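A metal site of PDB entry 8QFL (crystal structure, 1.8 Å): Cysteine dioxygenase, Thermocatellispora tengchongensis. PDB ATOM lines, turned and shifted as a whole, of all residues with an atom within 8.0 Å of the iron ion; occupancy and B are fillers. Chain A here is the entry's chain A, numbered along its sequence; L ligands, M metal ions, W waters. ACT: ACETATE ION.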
ATOM      1  N   THR A  85      26.482  13.508 -24.644  1.00  0.00           N
ATOM      2  CA  THR A  85      27.084  13.788 -23.342  1.00  0.00           C
ATOM      3  C   THR A  85      26.975  12.590 -22.410  1.00  0.00           C
ATOM      4  O   THR A  85      27.651  12.559 -21.359  1.00  0.00           O
ATOM      5  CB  THR A  85      26.444  14.994 -22.644  1.00  0.00           C
ATOM      6  OG1 THR A  85      25.078  14.726 -22.431  1.00  0.00           O
ATOM      7  CG2 THR A  85      26.644  16.295 -23.468  1.00  0.00           C
ATOM      8  N   GLY A  86      26.072  11.676 -22.683  1.00  0.00           N
ATOM      9  CA  GLY A  86      25.591  10.808 -21.584  1.00  0.00           C
ATOM     10  C   GLY A  86      24.705  11.485 -20.560  1.00  0.00           C
ATOM     11  O   GLY A  86      24.578  12.702 -20.542  1.00  0.00           O
ATOM     12  N   TRP A  87      24.085  10.704 -19.684  1.00  0.00           N
ATOM     13  CA  TRP A  87      23.297  11.277 -18.602  1.00  0.00           C
ATOM     14  C   TRP A  87      24.219  11.797 -17.521  1.00  0.00           C
ATOM     15  O   TRP A  87      25.132  11.069 -17.133  1.00  0.00           O
ATOM     16  CB  TRP A  87      22.406  10.191 -17.999  1.00  0.00           C
ATOM     17  CG  TRP A  87      21.323   9.735 -18.941  1.00  0.00           C
ATOM     18  CD1 TRP A  87      21.290   8.547 -19.606  1.00  0.00           C
ATOM     19  CD2 TRP A  87      20.108  10.438 -19.277  1.00  0.00           C
ATOM     20  NE1 TRP A  87      20.089   8.429 -20.302  1.00  0.00           N
ATOM     21  CE2 TRP A  87      19.378   9.604 -20.151  1.00  0.00           C
ATOM     22  CE3 TRP A  87      19.592  11.691 -18.964  1.00  0.00           C
ATOM     23  CZ2 TRP A  87      18.184   9.997 -20.715  1.00  0.00           C
ATOM     24  CZ3 TRP A  87      18.385  12.075 -19.501  1.00  0.00           C
ATOM     25  CH2 TRP A  87      17.678  11.217 -20.337  1.00  0.00           C
ATOM     26  N   HIS A  88      24.033  13.048 -17.097  1.00  0.00           N
ATOM     27  CA  HIS A  88      24.935  13.629 -16.115  1.00  0.00           C
ATOM     28  C   HIS A  88      24.249  14.708 -15.320  1.00  0.00           C
ATOM     29  O   HIS A  88      23.218  15.272 -15.738  1.00  0.00           O
ATOM     30  CB  HIS A  88      26.209  14.141 -16.735  1.00  0.00           C
ATOM     31  CG  HIS A  88      25.933  15.332 -17.657  1.00  0.00           C
ATOM     32  ND1 HIS A  88      25.449  15.173 -18.941  1.00  0.00           N
ATOM     33  CD2 HIS A  88      26.007  16.680 -17.462  1.00  0.00           C
ATOM     34  CE1 HIS A  88      25.247  16.354 -19.498  1.00  0.00           C
ATOM     35  NE2 HIS A  88      25.601  17.289 -18.647  1.00  0.00           N
ATOM     36  N   ASP A  89      24.832  15.015 -14.168  1.00  0.00           N
ATOM     37  CA  ASP A  89      24.518  16.213 -13.407  1.00  0.00           C
ATOM     38  C   ASP A  89      25.791  17.013 -13.291  1.00  0.00           C
ATOM     39  O   ASP A  89      26.853  16.574 -13.753  1.00  0.00           O
ATOM     40  CB  ASP A  89      23.944  15.883 -12.009  1.00  0.00           C
ATOM     41  CG  ASP A  89      24.968  15.184 -11.147  1.00  0.00           C
ATOM     42  OD1 ASP A  89      26.008  15.820 -10.739  1.00  0.00           O
ATOM     43  OD2 ASP A  89      24.698  13.985 -10.834  1.00  0.00           O
ATOM     44  N   HIS A  90      25.625  18.249 -12.778  1.00  0.00           N
ATOM     45  CA  HIS A  90      26.715  19.223 -12.699  1.00  0.00           C
ATOM     46  C   HIS A  90      27.115  19.488 -11.262  1.00  0.00           C
ATOM     47  O   HIS A  90      27.671  20.555 -10.955  1.00  0.00           O
ATOM     48  CB  HIS A  90      26.275  20.525 -13.367  1.00  0.00           C
ATOM     49  CG  HIS A  90      25.689  20.259 -14.704  1.00  0.00           C
ATOM     50  ND1 HIS A  90      24.336  20.157 -14.906  1.00  0.00           N
ATOM     51  CD2 HIS A  90      26.274  19.914 -15.869  1.00  0.00           C
ATOM     52  CE1 HIS A  90      24.110  19.816 -16.165  1.00  0.00           C
ATOM     53  NE2 HIS A  90      25.277  19.713 -16.773  1.00  0.00           N
ATOM     54  N   GLY A  95      23.565  26.081 -14.671  1.00  0.00           N
ATOM     55  CA  GLY A  95      24.060  26.163 -16.042  1.00  0.00           C
ATOM     56  C   GLY A  95      23.048  26.784 -16.977  1.00  0.00           C
ATOM     57  O   GLY A  95      21.865  26.936 -16.678  1.00  0.00           O
ATOM     58  N   VAL A  97      22.478  27.059 -21.597  1.00  0.00           N
ATOM     59  CA  VAL A  97      22.879  26.686 -22.951  1.00  0.00           C
ATOM     60  C   VAL A  97      22.190  27.618 -23.932  1.00  0.00           C
ATOM     61  O   VAL A  97      21.003  27.915 -23.777  1.00  0.00           O
ATOM     62  CB  VAL A  97      22.515  25.222 -23.289  1.00  0.00           C
ATOM     63  CG1 VAL A  97      22.935  24.846 -24.676  1.00  0.00           C
ATOM     64  CG2 VAL A  97      23.216  24.259 -22.229  1.00  0.00           C
ATOM     65  N   GLU A 106      17.781  18.107 -25.832  1.00  0.00           N
ATOM     66  CA  GLU A 106      17.934  18.125 -24.391  1.00  0.00           C
ATOM     67  C   GLU A 106      17.014  17.014 -23.888  1.00  0.00           C
ATOM     68  O   GLU A 106      15.807  17.095 -24.113  1.00  0.00           O
ATOM     69  CB  GLU A 106      17.569  19.489 -23.806  1.00  0.00           C
ATOM     70  CG  GLU A 106      17.083  19.527 -22.346  1.00  0.00           C
ATOM     71  CD  GLU A 106      18.242  19.545 -21.333  1.00  0.00           C
ATOM     72  OE1 GLU A 106      18.042  19.824 -20.125  1.00  0.00           O
ATOM     73  OE2 GLU A 106      19.375  19.312 -21.788  1.00  0.00           O
ATOM     74  N   PHE A 126      18.246  27.810 -22.716  1.00  0.00           N
ATOM     75  CA  PHE A 126      17.554  27.380 -21.510  1.00  0.00           C
ATOM     76  C   PHE A 126      18.591  27.363 -20.379  1.00  0.00           C
ATOM     77  O   PHE A 126      19.802  27.460 -20.621  1.00  0.00           O
ATOM     78  CB  PHE A 126      16.901  25.987 -21.652  1.00  0.00           C
ATOM     79  CG  PHE A 126      17.861  24.898 -21.926  1.00  0.00           C
ATOM     80  CD1 PHE A 126      18.287  24.653 -23.196  1.00  0.00           C
ATOM     81  CD2 PHE A 126      18.346  24.131 -20.887  1.00  0.00           C
ATOM     82  CE1 PHE A 126      19.199  23.605 -23.493  1.00  0.00           C
ATOM     83  CE2 PHE A 126      19.277  23.071 -21.140  1.00  0.00           C
ATOM     84  CZ  PHE A 126      19.665  22.795 -22.412  1.00  0.00           C
ATOM     85  N   PHE A 128      19.242  26.024 -15.957  1.00  0.00           N
ATOM     86  CA  PHE A 128      18.815  25.035 -14.980  1.00  0.00           C
ATOM     87  C   PHE A 128      19.604  25.292 -13.720  1.00  0.00           C
ATOM     88  O   PHE A 128      20.682  25.877 -13.756  1.00  0.00           O
ATOM     89  CB  PHE A 128      19.046  23.612 -15.440  1.00  0.00           C
ATOM     90  CG  PHE A 128      20.373  23.357 -16.027  1.00  0.00           C
ATOM     91  CD1 PHE A 128      21.456  23.119 -15.244  1.00  0.00           C
ATOM     92  CD2 PHE A 128      20.535  23.339 -17.450  1.00  0.00           C
ATOM     93  CE1 PHE A 128      22.704  22.929 -15.825  1.00  0.00           C
ATOM     94  CE2 PHE A 128      21.760  23.098 -17.971  1.00  0.00           C
ATOM     95  CZ  PHE A 128      22.848  22.930 -17.138  1.00  0.00           C
ATOM     96  N   HIS A 132      19.853  19.653 -11.663  1.00  0.00           N
ATOM     97  CA  HIS A 132      19.460  19.142 -12.964  1.00  0.00           C
ATOM     98  C   HIS A 132      20.215  17.883 -13.369  1.00  0.00           C
ATOM     99  O   HIS A 132      21.442  17.832 -13.227  1.00  0.00           O
ATOM    100  CB  HIS A 132      19.751  20.268 -13.978  1.00  0.00           C
ATOM    101  CG  HIS A 132      19.031  20.153 -15.275  1.00  0.00           C
ATOM    102  ND1 HIS A 132      17.667  20.217 -15.380  1.00  0.00           N
ATOM    103  CD2 HIS A 132      19.511  20.011 -16.526  1.00  0.00           C
ATOM    104  CE1 HIS A 132      17.331  20.128 -16.655  1.00  0.00           C
ATOM    105  NE2 HIS A 132      18.433  20.045 -17.381  1.00  0.00           N
ATOM    106  N   ILE A 133      19.481  16.893 -13.912  1.00  0.00           N
ATOM    107  CA  ILE A 133      20.056  15.734 -14.588  1.00  0.00           C
ATOM    108  C   ILE A 133      19.585  15.777 -16.038  1.00  0.00           C
ATOM    109  O   ILE A 133      18.385  15.852 -16.300  1.00  0.00           O
ATOM    110  CB  ILE A 133      19.654  14.371 -13.986  1.00  0.00           C
ATOM    111  CG1 ILE A 133      19.969  14.349 -12.499  1.00  0.00           C
ATOM    112  CG2 ILE A 133      20.365  13.248 -14.753  1.00  0.00           C
ATOM    113  CD1 ILE A 133      19.303  13.130 -11.714  1.00  0.00           C
ATOM    114  N   HIS A 134      20.515  15.666 -16.964  1.00  0.00           N
ATOM    115  CA  HIS A 134      20.184  15.782 -18.382  1.00  0.00           C
ATOM    116  C   HIS A 134      21.163  15.072 -19.268  1.00  0.00           C
ATOM    117  O   HIS A 134      22.208  14.600 -18.821  1.00  0.00           O
ATOM    118  CB  HIS A 134      20.015  17.273 -18.757  1.00  0.00           C
ATOM    119  CG  HIS A 134      21.289  18.030 -18.985  1.00  0.00           C
ATOM    120  ND1 HIS A 134      21.308  19.148 -19.817  1.00  0.00           N
ATOM    121  CD2 HIS A 134      22.556  17.924 -18.485  1.00  0.00           C
ATOM    122  CE1 HIS A 134      22.545  19.634 -19.895  1.00  0.00           C
ATOM    123  NE2 HIS A 134      23.316  18.969 -19.055  1.00  0.00           N
ATOM    124  N   ARG A 135      20.834  15.091 -20.575  1.00  0.00           N
ATOM    125  CA  ARG A 135      21.623  14.463 -21.572  1.00  0.00           C
ATOM    126  C   ARG A 135      21.424  15.313 -22.841  1.00  0.00           C
ATOM    127  O   ARG A 135      20.278  15.614 -23.157  1.00  0.00           O
ATOM    128  CB  ARG A 135      21.137  13.062 -21.844  1.00  0.00           C
ATOM    129  CG  ARG A 135      21.827  12.404 -22.934  1.00  0.00           C
ATOM    130  CD  ARG A 135      21.626  10.880 -22.846  1.00  0.00           C
ATOM    131  NE  ARG A 135      22.045  10.236 -24.075  1.00  0.00           N
ATOM    132  CZ  ARG A 135      21.283   9.336 -24.737  1.00  0.00           C
ATOM    133  NH1 ARG A 135      20.054   9.002 -24.290  1.00  0.00           N
ATOM    134  NH2 ARG A 135      21.735   8.790 -25.862  1.00  0.00           N
ATOM    135  N   LEU A 136      22.501  15.660 -23.485  1.00  0.00           N
ATOM    136  CA  LEU A 136      22.452  16.389 -24.776  1.00  0.00           C
ATOM    137  C   LEU A 136      22.963  15.464 -25.847  1.00  0.00           C
ATOM    138  O   LEU A 136      24.079  14.947 -25.719  1.00  0.00           O
ATOM    139  CB  LEU A 136      23.342  17.635 -24.686  1.00  0.00           C
ATOM    140  CG  LEU A 136      22.715  18.873 -24.049  1.00  0.00           C
ATOM    141  CD1 LEU A 136      21.877  18.666 -23.030  1.00  0.00           C
ATOM    142  CD2 LEU A 136      23.874  19.935 -23.737  1.00  0.00           C
ATOM    143  N   HIS A 147      27.890  27.163 -23.588  1.00  0.00           N
ATOM    144  CA  HIS A 147      27.481  26.595 -22.305  1.00  0.00           C
ATOM    145  C   HIS A 147      28.179  27.377 -21.178  1.00  0.00           C
ATOM    146  O   HIS A 147      29.374  27.553 -21.245  1.00  0.00           O
ATOM    147  CB  HIS A 147      27.804  25.105 -22.184  1.00  0.00           C
ATOM    148  CG  HIS A 147      27.290  24.292 -23.336  1.00  0.00           C
ATOM    149  ND1 HIS A 147      26.418  23.249 -23.166  1.00  0.00           N
ATOM    150  CD2 HIS A 147      27.414  24.455 -24.683  1.00  0.00           C
ATOM    151  CE1 HIS A 147      26.033  22.783 -24.338  1.00  0.00           C
ATOM    152  NE2 HIS A 147      26.637  23.475 -25.287  1.00  0.00           N
ATOM    153  N   TYR A 149      28.510  27.877 -16.774  1.00  0.00           N
ATOM    154  CA  TYR A 149      28.262  27.227 -15.478  1.00  0.00           C
ATOM    155  C   TYR A 149      28.744  28.141 -14.395  1.00  0.00           C
ATOM    156  O   TYR A 149      29.821  28.717 -14.539  1.00  0.00           O
ATOM    157  CB  TYR A 149      29.045  25.917 -15.376  1.00  0.00           C
ATOM    158  CG  TYR A 149      28.758  24.946 -16.473  1.00  0.00           C
ATOM    159  CD1 TYR A 149      29.508  24.934 -17.670  1.00  0.00           C
ATOM    160  CD2 TYR A 149      27.745  24.032 -16.344  1.00  0.00           C
ATOM    161  CE1 TYR A 149      29.238  24.120 -18.680  1.00  0.00           C
ATOM    162  CE2 TYR A 149      27.467  23.165 -17.430  1.00  0.00           C
ATOM    163  CZ  TYR A 149      28.222  23.171 -18.513  1.00  0.00           C
ATOM    164  OH  TYR A 149      27.922  22.277 -19.537  1.00  0.00           O
ATOM    165  N   LEU A 153      32.247  24.380 -13.250  1.00  0.00           N
ATOM    166  CA  LEU A 153      32.017  22.947 -13.464  1.00  0.00           C
ATOM    167  C   LEU A 153      33.307  22.216 -13.127  1.00  0.00           C
ATOM    168  O   LEU A 153      34.066  21.801 -13.983  1.00  0.00           O
ATOM    169  CB  LEU A 153      31.568  22.698 -14.903  1.00  0.00           C
ATOM    170  CG  LEU A 153      31.068  21.288 -15.149  1.00  0.00           C
ATOM    171  CD1 LEU A 153      29.806  21.084 -14.307  1.00  0.00           C
ATOM    172  CD2 LEU A 153      30.804  21.078 -16.644  1.00  0.00           C
ATOM    173  N   LEU A 156      31.458  16.772 -12.128  1.00  0.00           N
ATOM    174  CA  LEU A 156      30.290  16.278 -12.877  1.00  0.00           C
ATOM    175  C   LEU A 156      29.937  14.851 -12.402  1.00  0.00           C
ATOM    176  O   LEU A 156      30.813  14.061 -12.111  1.00  0.00           O
ATOM    177  CB  LEU A 156      30.643  16.238 -14.284  1.00  0.00           C
ATOM    178  CG  LEU A 156      29.669  15.768 -15.338  1.00  0.00           C
ATOM    179  CD1 LEU A 156      29.659  16.886 -16.451  1.00  0.00           C
ATOM    180  CD2 LEU A 156      30.161  14.493 -15.862  1.00  0.00           C
HETATM  181  C   ACT L   1      25.174  22.217 -19.989  1.00  0.00           C
HETATM  182  O   ACT L   1      25.068  21.459 -18.952  1.00  0.00           O
HETATM  183  OXT ACT L   1      25.289  21.945 -21.176  1.00  0.00           O
HETATM  184  CH3 ACT L   1      25.158  23.729 -19.669  1.00  0.00           C
HETATM  185 FE    FE M   1      25.266  19.294 -18.810  1.00  0.00          FE
HETATM  186  O   HOH W   1      27.325  19.602 -18.838  1.00  0.00           O
HETATM  187  O   HOH W   2      25.692  19.238 -21.094  1.00  0.00           O
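ND1 of His 134 lies within hydrogen-bond range of OE2 of Glu 106.
ND1 of His 88 sits at hydrogen-bond distance from O of Gly 86 (3.1 Å).
The nearest printed residue that does not touch the iron ion is Tyr 149 (4.1 Å).
NE2 of His 134 is bound to the iron ion (2.0 Å).
The iron ion is bound by a ring nitrogen (NE2) of His 88.
The iron ion is bound by a ring nitrogen (NE2) of His 90, at 2.1 Å.
The iron ion is bound by water W1, at 2.1 Å.
O of the ligand is bound to the iron ion.
The iron ion is bound by water W2 (2.3 Å).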
